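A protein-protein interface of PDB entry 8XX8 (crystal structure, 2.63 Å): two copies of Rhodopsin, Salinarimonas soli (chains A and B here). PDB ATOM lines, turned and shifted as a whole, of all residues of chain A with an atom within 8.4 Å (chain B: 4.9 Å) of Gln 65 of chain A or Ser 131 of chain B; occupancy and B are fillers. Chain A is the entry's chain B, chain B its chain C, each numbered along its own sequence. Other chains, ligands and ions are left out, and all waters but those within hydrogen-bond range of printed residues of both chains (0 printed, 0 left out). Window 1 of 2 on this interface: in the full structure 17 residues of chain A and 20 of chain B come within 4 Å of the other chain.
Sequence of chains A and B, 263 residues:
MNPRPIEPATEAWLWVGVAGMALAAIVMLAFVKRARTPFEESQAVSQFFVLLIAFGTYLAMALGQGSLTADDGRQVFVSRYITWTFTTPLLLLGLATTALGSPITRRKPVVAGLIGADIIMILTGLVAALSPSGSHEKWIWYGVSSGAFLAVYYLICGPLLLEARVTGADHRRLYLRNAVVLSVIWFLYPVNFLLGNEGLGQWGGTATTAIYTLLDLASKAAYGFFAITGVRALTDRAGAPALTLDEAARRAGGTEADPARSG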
ATOM      1  N   MET A   1       1.125 -24.251 -25.553  1.00  0.00           N
ATOM      2  CA  MET A   1       2.292 -23.424 -25.798  1.00  0.00           C
ATOM      3  C   MET A   1       2.578 -23.254 -27.286  1.00  0.00           C
ATOM      4  O   MET A   1       3.658 -23.609 -27.753  1.00  0.00           O
ATOM      5  CB  MET A   1       3.506 -24.025 -25.105  1.00  0.00           C
ATOM      6  CG  MET A   1       3.444 -23.923 -23.595  1.00  0.00           C
ATOM      7  SD  MET A   1       5.087 -23.896 -22.833  1.00  0.00           S
ATOM      8  CE  MET A   1       5.812 -22.543 -23.754  1.00  0.00           C
ATOM      9  N   ASN A   2       1.607 -22.760 -28.018  1.00  0.00           N
ATOM     10  CA  ASN A   2       1.872 -22.460 -29.422  1.00  0.00           C
ATOM     11  C   ASN A   2       2.526 -21.088 -29.534  1.00  0.00           C
ATOM     12  O   ASN A   2       2.096 -20.130 -28.870  1.00  0.00           O
ATOM     13  CB  ASN A   2       0.595 -22.499 -30.257  1.00  0.00           C
ATOM     14  CG  ASN A   2       0.054 -23.916 -30.384  1.00  0.00           C
ATOM     15  OD1 ASN A   2       0.326 -24.763 -29.538  1.00  0.00           O
ATOM     16  ND2 ASN A   2      -0.713 -24.183 -31.452  1.00  0.00           N
ATOM     17  N   PRO A   3       3.525 -20.945 -30.404  1.00  0.00           N
ATOM     18  CA  PRO A   3       4.280 -19.689 -30.456  1.00  0.00           C
ATOM     19  C   PRO A   3       3.455 -18.510 -30.900  1.00  0.00           C
ATOM     20  O   PRO A   3       2.716 -18.593 -31.872  1.00  0.00           O
ATOM     21  CB  PRO A   3       5.387 -19.984 -31.462  1.00  0.00           C
ATOM     22  CG  PRO A   3       5.394 -21.479 -31.654  1.00  0.00           C
ATOM     23  CD  PRO A   3       4.009 -21.936 -31.380  1.00  0.00           C
ATOM     24  N   ARG A   4       3.643 -17.376 -30.182  1.00  0.00           N
ATOM     25  CA  ARG A   4       3.078 -16.066 -30.465  1.00  0.00           C
ATOM     26  C   ARG A   4       4.125 -15.196 -31.146  1.00  0.00           C
ATOM     27  O   ARG A   4       5.243 -15.059 -30.617  1.00  0.00           O
ATOM     28  CB  ARG A   4       2.609 -15.403 -29.171  1.00  0.00           C
ATOM     29  CG  ARG A   4       1.364 -16.020 -28.563  1.00  0.00           C
ATOM     30  CD  ARG A   4       1.696 -17.175 -27.629  1.00  0.00           C
ATOM     31  NE  ARG A   4       0.504 -17.919 -27.226  1.00  0.00           N
ATOM     32  CZ  ARG A   4      -0.200 -17.675 -26.122  1.00  0.00           C
ATOM     33  NH1 ARG A   4      -1.269 -18.409 -25.840  1.00  0.00           N
ATOM     34  NH2 ARG A   4       0.164 -16.699 -25.301  1.00  0.00           N
ATOM     35  N   PRO A   5       3.807 -14.600 -32.296  1.00  0.00           N
ATOM     36  CA  PRO A   5       4.827 -13.870 -33.056  1.00  0.00           C
ATOM     37  C   PRO A   5       5.335 -12.646 -32.308  1.00  0.00           C
ATOM     38  O   PRO A   5       4.628 -12.046 -31.495  1.00  0.00           O
ATOM     39  CB  PRO A   5       4.094 -13.474 -34.337  1.00  0.00           C
ATOM     40  CG  PRO A   5       2.943 -14.441 -34.438  1.00  0.00           C
ATOM     41  CD  PRO A   5       2.533 -14.713 -33.025  1.00  0.00           C
ATOM     42  N   ILE A   6       6.581 -12.278 -32.604  1.00  0.00           N
ATOM     43  CA  ILE A   6       7.251 -11.143 -31.986  1.00  0.00           C
ATOM     44  C   ILE A   6       7.665 -10.169 -33.083  1.00  0.00           C
ATOM     45  O   ILE A   6       7.742 -10.519 -34.263  1.00  0.00           O
ATOM     46  CB  ILE A   6       8.480 -11.573 -31.154  1.00  0.00           C
ATOM     47  CG1 ILE A   6       8.241 -12.933 -30.494  1.00  0.00           C
ATOM     48  CG2 ILE A   6       8.805 -10.538 -30.088  1.00  0.00           C
ATOM     49  CD1 ILE A   6       7.260 -12.893 -29.343  1.00  0.00           C
ATOM     50  N   LEU A  14      16.688 -11.177 -29.252  1.00  0.00           N
ATOM     51  CA  LEU A  14      16.547 -12.395 -28.462  1.00  0.00           C
ATOM     52  C   LEU A  14      17.456 -13.499 -28.985  1.00  0.00           C
ATOM     53  O   LEU A  14      18.007 -14.279 -28.199  1.00  0.00           O
ATOM     54  CB  LEU A  14      15.091 -12.854 -28.457  1.00  0.00           C
ATOM     55  CG  LEU A  14      14.105 -11.956 -27.711  1.00  0.00           C
ATOM     56  CD1 LEU A  14      12.674 -12.369 -28.016  1.00  0.00           C
ATOM     57  CD2 LEU A  14      14.373 -12.004 -26.212  1.00  0.00           C
ATOM     58  N   GLY A  56      18.324 -21.261 -22.252  1.00  0.00           N
ATOM     59  CA  GLY A  56      17.009 -21.827 -22.493  1.00  0.00           C
ATOM     60  C   GLY A  56      15.900 -20.795 -22.437  1.00  0.00           C
ATOM     61  O   GLY A  56      14.920 -20.885 -23.183  1.00  0.00           O
ATOM     62  N   THR A  57      16.032 -19.799 -21.557  1.00  0.00           N
ATOM     63  CA  THR A  57      14.982 -18.791 -21.454  1.00  0.00           C
ATOM     64  C   THR A  57      15.000 -17.854 -22.658  1.00  0.00           C
ATOM     65  O   THR A  57      13.941 -17.437 -23.142  1.00  0.00           O
ATOM     66  CB  THR A  57      15.105 -18.013 -20.139  1.00  0.00           C
ATOM     67  OG1 THR A  57      13.886 -17.300 -19.885  1.00  0.00           O
ATOM     68  CG2 THR A  57      16.267 -17.023 -20.163  1.00  0.00           C
ATOM     69  N   TYR A  58      16.188 -17.532 -23.175  1.00  0.00           N
ATOM     70  CA  TYR A  58      16.245 -16.748 -24.400  1.00  0.00           C
ATOM     71  C   TYR A  58      15.829 -17.582 -25.600  1.00  0.00           C
ATOM     72  O   TYR A  58      15.261 -17.046 -26.559  1.00  0.00           O
ATOM     73  CB  TYR A  58      17.644 -16.163 -24.591  1.00  0.00           C
ATOM     74  CG  TYR A  58      17.831 -14.863 -23.845  1.00  0.00           C
ATOM     75  CD1 TYR A  58      17.489 -13.652 -24.433  1.00  0.00           C
ATOM     76  CD2 TYR A  58      18.326 -14.847 -22.545  1.00  0.00           C
ATOM     77  CE1 TYR A  58      17.646 -12.459 -23.756  1.00  0.00           C
ATOM     78  CE2 TYR A  58      18.486 -13.657 -21.859  1.00  0.00           C
ATOM     79  CZ  TYR A  58      18.144 -12.467 -22.470  1.00  0.00           C
ATOM     80  OH  TYR A  58      18.300 -11.278 -21.797  1.00  0.00           O
ATOM     81  N   LEU A  59      16.089 -18.891 -25.563  1.00  0.00           N
ATOM     82  CA  LEU A  59      15.547 -19.775 -26.586  1.00  0.00           C
ATOM     83  C   LEU A  59      14.027 -19.783 -26.540  1.00  0.00           C
ATOM     84  O   LEU A  59      13.364 -19.709 -27.582  1.00  0.00           O
ATOM     85  CB  LEU A  59      16.101 -21.188 -26.409  1.00  0.00           C
ATOM     86  CG  LEU A  59      15.581 -22.251 -27.381  1.00  0.00           C
ATOM     87  CD1 LEU A  59      15.832 -21.840 -28.824  1.00  0.00           C
ATOM     88  CD2 LEU A  59      16.217 -23.601 -27.086  1.00  0.00           C
ATOM     89  N   ALA A  60      13.456 -19.852 -25.334  1.00  0.00           N
ATOM     90  CA  ALA A  60      12.003 -19.832 -25.195  1.00  0.00           C
ATOM     91  C   ALA A  60      11.422 -18.501 -25.650  1.00  0.00           C
ATOM     92  O   ALA A  60      10.363 -18.466 -26.288  1.00  0.00           O
ATOM     93  CB  ALA A  60      11.611 -20.124 -23.747  1.00  0.00           C
ATOM     94  N   MET A  61      12.099 -17.394 -25.336  1.00  0.00           N
ATOM     95  CA  MET A  61      11.622 -16.088 -25.778  1.00  0.00           C
ATOM     96  C   MET A  61      11.803 -15.908 -27.281  1.00  0.00           C
ATOM     97  O   MET A  61      10.941 -15.327 -27.950  1.00  0.00           O
ATOM     98  CB  MET A  61      12.338 -14.977 -25.011  1.00  0.00           C
ATOM     99  CG  MET A  61      11.871 -14.819 -23.574  1.00  0.00           C
ATOM    100  SD  MET A  61      12.660 -13.445 -22.714  1.00  0.00           S
ATOM    101  CE  MET A  61      14.305 -14.098 -22.451  1.00  0.00           C
ATOM    102  N   ALA A  62      12.918 -16.397 -27.833  1.00  0.00           N
ATOM    103  CA  ALA A  62      13.146 -16.254 -29.269  1.00  0.00           C
ATOM    104  C   ALA A  62      12.175 -17.103 -30.079  1.00  0.00           C
ATOM    105  O   ALA A  62      11.762 -16.698 -31.172  1.00  0.00           O
ATOM    106  CB  ALA A  62      14.589 -16.620 -29.615  1.00  0.00           C
ATOM    107  N   LEU A  63      11.795 -18.272 -29.564  1.00  0.00           N
ATOM    108  CA  LEU A  63      10.816 -19.107 -30.245  1.00  0.00           C
ATOM    109  C   LEU A  63       9.394 -18.584 -30.103  1.00  0.00           C
ATOM    110  O   LEU A  63       8.467 -19.225 -30.611  1.00  0.00           O
ATOM    111  CB  LEU A  63      10.898 -20.540 -29.718  1.00  0.00           C
ATOM    112  CG  LEU A  63      12.196 -21.293 -30.025  1.00  0.00           C
ATOM    113  CD1 LEU A  63      12.207 -22.657 -29.348  1.00  0.00           C
ATOM    114  CD2 LEU A  63      12.412 -21.428 -31.528  1.00  0.00           C
ATOM    115  N   GLY A  64       9.197 -17.447 -29.442  1.00  0.00           N
ATOM    116  CA  GLY A  64       7.860 -16.930 -29.228  1.00  0.00           C
ATOM    117  C   GLY A  64       7.056 -17.677 -28.191  1.00  0.00           C
ATOM    118  O   GLY A  64       5.827 -17.578 -28.187  1.00  0.00           O
ATOM    119  N   GLN A  65       7.717 -18.420 -27.301  1.00  0.00           N
ATOM    120  CA  GLN A  65       7.040 -19.260 -26.321  1.00  0.00           C
ATOM    121  C   GLN A  65       7.338 -18.835 -24.886  1.00  0.00           C
ATOM    122  O   GLN A  65       7.144 -19.626 -23.959  1.00  0.00           O
ATOM    123  CB  GLN A  65       7.422 -20.727 -26.523  1.00  0.00           C
ATOM    124  CG  GLN A  65       7.017 -21.299 -27.872  1.00  0.00           C
ATOM    125  CD  GLN A  65       7.397 -22.758 -28.016  1.00  0.00           C
ATOM    126  OE1 GLN A  65       8.575 -23.098 -28.134  1.00  0.00           O
ATOM    127  NE2 GLN A  65       6.397 -23.632 -28.003  1.00  0.00           N
ATOM    128  N   GLY A  66       7.802 -17.605 -24.681  1.00  0.00           N
ATOM    129  CA  GLY A  66       8.166 -17.167 -23.349  1.00  0.00           C
ATOM    130  C   GLY A  66       7.601 -15.817 -22.957  1.00  0.00           C
ATOM    131  O   GLY A  66       8.114 -15.166 -22.042  1.00  0.00           O
ATOM    132  N   SER A  67       6.548 -15.381 -23.638  1.00  0.00           N
ATOM    133  CA  SER A  67       5.922 -14.101 -23.359  1.00  0.00           C
ATOM    134  C   SER A  67       4.479 -14.314 -22.921  1.00  0.00           C
ATOM    135  O   SER A  67       3.908 -15.399 -23.061  1.00  0.00           O
ATOM    136  CB  SER A  67       5.983 -13.172 -24.582  1.00  0.00           C
ATOM    137  OG  SER A  67       5.078 -13.584 -25.592  1.00  0.00           O
ATOM    138  N   LEU A  68       3.891 -13.251 -22.379  1.00  0.00           N
ATOM    139  CA  LEU A  68       2.527 -13.281 -21.878  1.00  0.00           C
ATOM    140  C   LEU A  68       1.855 -11.961 -22.212  1.00  0.00           C
ATOM    141  O   LEU A  68       2.512 -10.922 -22.312  1.00  0.00           O
ATOM    142  CB  LEU A  68       2.492 -13.519 -20.363  1.00  0.00           C
ATOM    143  CG  LEU A  68       1.445 -14.486 -19.817  1.00  0.00           C
ATOM    144  CD1 LEU A  68       1.755 -15.908 -20.265  1.00  0.00           C
ATOM    145  CD2 LEU A  68       1.381 -14.397 -18.301  1.00  0.00           C
ATOM    146  N   GLN A  75       2.774  -6.826 -23.644  1.00  0.00           N
ATOM    147  CA  GLN A  75       3.440  -8.115 -23.779  1.00  0.00           C
ATOM    148  C   GLN A  75       4.600  -8.155 -22.795  1.00  0.00           C
ATOM    149  O   GLN A  75       5.476  -7.283 -22.827  1.00  0.00           O
ATOM    150  CB  GLN A  75       3.934  -8.331 -25.210  1.00  0.00           C
ATOM    151  CG  GLN A  75       4.637  -9.659 -25.438  1.00  0.00           C
ATOM    152  CD  GLN A  75       5.149  -9.812 -26.861  1.00  0.00           C
ATOM    153  OE1 GLN A  75       5.333  -8.826 -27.576  1.00  0.00           O
ATOM    154  NE2 GLN A  75       5.376 -11.054 -27.279  1.00  0.00           N
ATOM    155  N   VAL A  76       4.600  -9.158 -21.919  1.00  0.00           N
ATOM    156  CA  VAL A  76       5.618  -9.318 -20.886  1.00  0.00           C
ATOM    157  C   VAL A  76       6.310 -10.658 -21.096  1.00  0.00           C
ATOM    158  O   VAL A  76       5.644 -11.695 -21.213  1.00  0.00           O
ATOM    159  CB  VAL A  76       5.015  -9.232 -19.470  1.00  0.00           C
ATOM    160  CG1 VAL A  76       6.079  -9.506 -18.414  1.00  0.00           C
ATOM    161  CG2 VAL A  76       4.373  -7.873 -19.244  1.00  0.00           C
ATOM    162  N   PHE A  77       7.642 -10.637 -21.136  1.00  0.00           N
ATOM    163  CA  PHE A  77       8.432 -11.857 -21.296  1.00  0.00           C
ATOM    164  C   PHE A  77       8.585 -12.517 -19.928  1.00  0.00           C
ATOM    165  O   PHE A  77       9.600 -12.384 -19.239  1.00  0.00           O
ATOM    166  CB  PHE A  77       9.780 -11.547 -21.933  1.00  0.00           C
ATOM    167  CG  PHE A  77       9.686 -11.131 -23.373  1.00  0.00           C
ATOM    168  CD1 PHE A  77       9.624 -12.082 -24.379  1.00  0.00           C
ATOM    169  CD2 PHE A  77       9.653  -9.792 -23.721  1.00  0.00           C
ATOM    170  CE1 PHE A  77       9.535 -11.703 -25.708  1.00  0.00           C
ATOM    171  CE2 PHE A  77       9.562  -9.408 -25.049  1.00  0.00           C
ATOM    172  CZ  PHE A  77       9.504 -10.366 -26.043  1.00  0.00           C
ATOM    173  N   VAL A  78       7.541 -13.254 -19.539  1.00  0.00           N
ATOM    174  CA  VAL A  78       7.520 -13.888 -18.224  1.00  0.00           C
ATOM    175  C   VAL A  78       8.615 -14.940 -18.102  1.00  0.00           C
ATOM    176  O   VAL A  78       9.079 -15.230 -16.992  1.00  0.00           O
ATOM    177  CB  VAL A  78       6.131 -14.490 -17.945  1.00  0.00           C
ATOM    178  CG1 VAL A  78       5.111 -13.383 -17.734  1.00  0.00           C
ATOM    179  CG2 VAL A  78       5.709 -15.397 -19.092  1.00  0.00           C
ATOM    180  N   SER A  79       9.042 -15.529 -19.224  1.00  0.00           N
ATOM    181  CA  SER A  79      10.127 -16.506 -19.181  1.00  0.00           C
ATOM    182  C   SER A  79      11.382 -15.906 -18.563  1.00  0.00           C
ATOM    183  O   SER A  79      12.106 -16.583 -17.822  1.00  0.00           O
ATOM    184  CB  SER A  79      10.424 -17.028 -20.588  1.00  0.00           C
ATOM    185  OG  SER A  79      11.514 -17.938 -20.581  1.00  0.00           O
ATOM    186  N   ILE A  82      10.837 -15.867 -14.878  1.00  0.00           N
ATOM    187  CA  ILE A  82      10.791 -17.219 -14.328  1.00  0.00           C
ATOM    188  C   ILE A  82      12.199 -17.752 -14.099  1.00  0.00           C
ATOM    189  O   ILE A  82      12.493 -18.346 -13.054  1.00  0.00           O
ATOM    190  CB  ILE A  82       9.978 -18.145 -15.252  1.00  0.00           C
ATOM    191  CG1 ILE A  82       8.494 -17.783 -15.197  1.00  0.00           C
ATOM    192  CG2 ILE A  82      10.188 -19.602 -14.876  1.00  0.00           C
ATOM    193  CD1 ILE A  82       7.653 -18.528 -16.213  1.00  0.00           C
ATOM    194  N   ASP B  72      -2.810 -26.565 -29.560  1.00  0.00           N
ATOM    195  CA  ASP B  72      -3.030 -27.301 -30.798  1.00  0.00           C
ATOM    196  C   ASP B  72      -4.217 -28.253 -30.716  1.00  0.00           C
ATOM    197  O   ASP B  72      -4.660 -28.752 -31.754  1.00  0.00           O
ATOM    198  CB  ASP B  72      -1.764 -28.074 -31.181  1.00  0.00           C
ATOM    199  CG  ASP B  72      -1.501 -29.255 -30.271  1.00  0.00           C
ATOM    200  OD1 ASP B  72      -1.957 -30.368 -30.599  1.00  0.00           O
ATOM    201  OD2 ASP B  72      -0.843 -29.073 -29.226  1.00  0.00           O
ATOM    202  N   ARG B  74      -4.493 -31.008 -28.337  1.00  0.00           N
ATOM    203  CA  ARG B  74      -4.229 -32.269 -27.661  1.00  0.00           C
ATOM    204  C   ARG B  74      -4.467 -32.153 -26.157  1.00  0.00           C
ATOM    205  O   ARG B  74      -4.427 -31.068 -25.569  1.00  0.00           O
ATOM    206  CB  ARG B  74      -2.795 -32.730 -27.916  1.00  0.00           C
ATOM    207  CG  ARG B  74      -2.548 -33.252 -29.313  1.00  0.00           C
ATOM    208  CD  ARG B  74      -1.105 -33.675 -29.497  1.00  0.00           C
ATOM    209  NE  ARG B  74      -0.182 -32.553 -29.349  1.00  0.00           N
ATOM    210  CZ  ARG B  74       0.570 -32.337 -28.274  1.00  0.00           C
ATOM    211  NH1 ARG B  74       0.515 -33.169 -27.244  1.00  0.00           N
ATOM    212  NH2 ARG B  74       1.380 -31.287 -28.231  1.00  0.00           N
ATOM    213  N   VAL B 127       7.605 -28.457 -22.164  1.00  0.00           N
ATOM    214  CA  VAL B 127       7.417 -27.498 -23.249  1.00  0.00           C
ATOM    215  C   VAL B 127       7.270 -28.223 -24.580  1.00  0.00           C
ATOM    216  O   VAL B 127       6.432 -27.858 -25.414  1.00  0.00           O
ATOM    217  CB  VAL B 127       8.579 -26.488 -23.279  1.00  0.00           C
ATOM    218  CG1 VAL B 127       8.421 -25.534 -24.451  1.00  0.00           C
ATOM    219  CG2 VAL B 127       8.647 -25.718 -21.969  1.00  0.00           C
ATOM    220  N   ALA B 128       8.078 -29.264 -24.799  1.00  0.00           N
ATOM    221  CA  ALA B 128       7.940 -30.058 -26.014  1.00  0.00           C
ATOM    222  C   ALA B 128       6.583 -30.751 -26.065  1.00  0.00           C
ATOM    223  O   ALA B 128       5.992 -30.898 -27.142  1.00  0.00           O
ATOM    224  CB  ALA B 128       9.072 -31.079 -26.104  1.00  0.00           C
ATOM    225  N   ALA B 129       6.068 -31.175 -24.907  1.00  0.00           N
ATOM    226  CA  ALA B 129       4.768 -31.834 -24.871  1.00  0.00           C
ATOM    227  C   ALA B 129       3.628 -30.858 -25.133  1.00  0.00           C
ATOM    228  O   ALA B 129       2.593 -31.252 -25.685  1.00  0.00           O
ATOM    229  CB  ALA B 129       4.570 -32.532 -23.526  1.00  0.00           C
ATOM    230  N   LEU B 130       3.791 -29.593 -24.749  1.00  0.00           N
ATOM    231  CA  LEU B 130       2.772 -28.577 -24.979  1.00  0.00           C
ATOM    232  C   LEU B 130       2.940 -27.852 -26.310  1.00  0.00           C
ATOM    233  O   LEU B 130       2.017 -27.149 -26.736  1.00  0.00           O
ATOM    234  CB  LEU B 130       2.775 -27.560 -23.833  1.00  0.00           C
ATOM    235  CG  LEU B 130       2.295 -28.084 -22.476  1.00  0.00           C
ATOM    236  CD1 LEU B 130       2.711 -27.149 -21.357  1.00  0.00           C
ATOM    237  CD2 LEU B 130       0.785 -28.278 -22.473  1.00  0.00           C
ATOM    238  N   SER B 131       4.083 -28.007 -26.974  1.00  0.00           N
ATOM    239  CA  SER B 131       4.276 -27.419 -28.288  1.00  0.00           C
ATOM    240  C   SER B 131       3.392 -28.130 -29.314  1.00  0.00           C
ATOM    241  O   SER B 131       3.001 -29.281 -29.113  1.00  0.00           O
ATOM    242  CB  SER B 131       5.746 -27.508 -28.690  1.00  0.00           C
ATOM    243  OG  SER B 131       6.562 -26.768 -27.802  1.00  0.00           O
ATOM    244  N   PRO B 132       3.062 -27.463 -30.422  1.00  0.00           N
ATOM    245  CA  PRO B 132       2.112 -28.051 -31.376  1.00  0.00           C
ATOM    246  C   PRO B 132       2.664 -29.298 -32.052  1.00  0.00           C
ATOM    247  O   PRO B 132       3.877 -29.484 -32.182  1.00  0.00           O
ATOM    248  CB  PRO B 132       1.887 -26.931 -32.401  1.00  0.00           C
ATOM    249  CG  PRO B 132       2.466 -25.698 -31.797  1.00  0.00           C
ATOM    250  CD  PRO B 132       3.527 -26.133 -30.854  1.00  0.00           C
ATOM    251  N   SER B 133       1.746 -30.156 -32.489  1.00  0.00           N
ATOM    252  CA  SER B 133       2.123 -31.329 -33.265  1.00  0.00           C
ATOM    253  C   SER B 133       2.582 -30.916 -34.657  1.00  0.00           C
ATOM    254  O   SER B 133       1.983 -30.045 -35.294  1.00  0.00           O
ATOM    255  CB  SER B 133       0.951 -32.303 -33.368  1.00  0.00           C
ATOM    256  OG  SER B 133       0.670 -32.901 -32.114  1.00  0.00           O
ATOM    257  N   SER B 135       5.182 -29.254 -35.369  1.00  0.00           N
ATOM    258  CA  SER B 135       5.931 -28.010 -35.319  1.00  0.00           C
ATOM    259  C   SER B 135       7.414 -28.292 -35.090  1.00  0.00           C
ATOM    260  O   SER B 135       7.820 -29.404 -34.744  1.00  0.00           O
ATOM    261  CB  SER B 135       5.389 -27.102 -34.214  1.00  0.00           C
ATOM    262  OG  SER B 135       5.658 -27.650 -32.935  1.00  0.00           O
ATOM    263  N   GLU B 137       9.155 -26.192 -32.923  1.00  0.00           N
ATOM    264  CA  GLU B 137       9.378 -25.882 -31.517  1.00  0.00           C
ATOM    265  C   GLU B 137       9.338 -27.144 -30.666  1.00  0.00           C
ATOM    266  O   GLU B 137      10.110 -27.285 -29.711  1.00  0.00           O
ATOM    267  CB  GLU B 137       8.341 -24.865 -31.035  1.00  0.00           C
ATOM    268  CG  GLU B 137       8.610 -23.420 -31.463  1.00  0.00           C
ATOM    269  CD  GLU B 137       8.308 -23.145 -32.929  1.00  0.00           C
ATOM    270  OE1 GLU B 137       7.791 -24.045 -33.625  1.00  0.00           O
ATOM    271  OE2 GLU B 137       8.590 -22.016 -33.387  1.00  0.00           O
ATOM    272  N   LYS B 138       8.467 -28.093 -31.026  1.00  0.00           N
ATOM    273  CA  LYS B 138       8.348 -29.327 -30.258  1.00  0.00           C
ATOM    274  C   LYS B 138       9.647 -30.120 -30.267  1.00  0.00           C
ATOM    275  O   LYS B 138      10.077 -30.633 -29.225  1.00  0.00           O
ATOM    276  CB  LYS B 138       7.202 -30.177 -30.809  1.00  0.00           C
ATOM    277  CG  LYS B 138       7.130 -31.582 -30.227  1.00  0.00           C
ATOM    278  CD  LYS B 138       6.040 -32.402 -30.900  1.00  0.00           C
ATOM    279  CE  LYS B 138       4.844 -32.621 -29.983  1.00  0.00           C
ATOM    280  NZ  LYS B 138       4.222 -31.351 -29.524  1.00  0.00           N
ATOM    281  N   TRP B 141      12.798 -28.404 -28.434  1.00  0.00           N
ATOM    282  CA  TRP B 141      12.764 -28.675 -26.999  1.00  0.00           C
ATOM    283  C   TRP B 141      12.922 -30.159 -26.699  1.00  0.00           C
ATOM    284  O   TRP B 141      13.498 -30.519 -25.666  1.00  0.00           O
ATOM    285  CB  TRP B 141      11.469 -28.139 -26.391  1.00  0.00           C
ATOM    286  CG  TRP B 141      11.412 -26.644 -26.380  1.00  0.00           C
ATOM    287  CD1 TRP B 141      10.564 -25.850 -27.096  1.00  0.00           C
ATOM    288  CD2 TRP B 141      12.255 -25.761 -25.632  1.00  0.00           C
ATOM    289  NE1 TRP B 141      10.819 -24.527 -26.830  1.00  0.00           N
ATOM    290  CE2 TRP B 141      11.853 -24.444 -25.935  1.00  0.00           C
ATOM    291  CE3 TRP B 141      13.308 -25.955 -24.731  1.00  0.00           C
ATOM    292  CZ2 TRP B 141      12.466 -23.329 -25.369  1.00  0.00           C
ATOM    293  CZ3 TRP B 141      13.915 -24.845 -24.172  1.00  0.00           C
ATOM    294  CH2 TRP B 141      13.493 -23.550 -24.493  1.00  0.00           C
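No position is printed for both chains.
Of the 13 pairs that touch across the chains among the printed residues, none has its exchanged pair printed and touching as well.
N of Met 1 of chain A lies within hydrogen-bond range of O of Leu 130 of chain B (3.3 Å).
The side-chain amide nitrogen (NE2) of Gln 65 of chain A is in hydrogen-bond range of the side-chain hydroxyl (OG) of Ser 131 of chain B (3.1 Å).
The side-chain amide oxygen of Gln 65 of chain A is in hydrogen-bond range of the indole nitrogen of Trp 141 of chain B (3.0 Å).
Of the 26 printed residues of chain A, 8 touch a printed residue of chain B.
Along chain B the printed residues that touch a printed residue of chain A span positions 72 to 141.
Among the printed residues, no Asp or Glu carboxylate lies within 4 Å of a Lys or Arg side-chain nitrogen of the other chain.
CA of Ser 131 of chain B touches O of Met 1 of chain A, at 3.9 Å.
Asp 72 of chain B touches Asn 2 of chain A.
OD1 of Asn 2 of chain A touches CG of Pro 132 of chain B (3.2 Å).
Glu 137 of chain B touches Pro 3 of chain A (CD to CG, 3.6 Å).
Trp 141 of chain B touches Gly 56 of chain A.
Leu 59 of chain A touches Trp 141 of chain B.
Ala 60 of chain A touches Trp 141 of chain B (CA to CZ2, 3.5 Å).
Leu 63 of chain A touches Glu 137 of chain B (O to OE2, 3.9 Å).
CD1 of Leu 63 of chain A touches NE1 of Trp 141 of chain B, at 3.4 Å.
OE1 of Gln 65 of chain A touches CG of Glu 137 of chain B (3.3 Å).
Of chain B, only Ser 131, Glu 137 and Trp 141 come within 4 Å of Gln 65 of chain A.
Printed residues of chain A within 4 Å of Ser 131 of chain B: Met 1 and Gln 65.
Printed residues of chain A within 4 Å of Asp 72 of chain B: Asn 2.
Printed residues of chain B within 4 Å of Asn 2 of chain A: Asp 72 and Pro 132.
Printed residues of chain A within 4 Å of Pro 132 of chain B: Asn 2.
Arg 74 of chain B touches none of the printed residues of chain A.
Ser 135 of chain B touches none of the printed residues of chain A.
The nearest residue of chain B that does not touch Gln 65 of chain A is Val 127 of chain B (4.4 Å).
The backbone carbonyl oxygen of Met 1 of chain A is in hydrogen-bond range of the side-chain amide nitrogen of Gln 65 of chain A (2.8 Å).
The backbone NH of Gly 66 of chain A is in hydrogen-bond range of the backbone carbonyl oxygen of Ala 60 of chain A.
The guanidinium group of Arg 74 of chain B sits at hydrogen-bond distance from the backbone carbonyl oxygen of Ser 131 of chain B (2.7 Å).
The backbone carbonyl oxygen of Val 127 of chain B lies within hydrogen-bond range of the side-chain hydroxyl of Ser 131 of chain B (2.6 Å).
O of Ser 131 of chain B sits at hydrogen-bond distance from NZ of Lys 138 of chain B, 2.4 Å away.
The side-chain hydroxyl (OG) of Ser 135 of chain B lies within hydrogen-bond range of the backbone carbonyl oxygen (O) of Pro 132 of chain B (2.7 Å).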
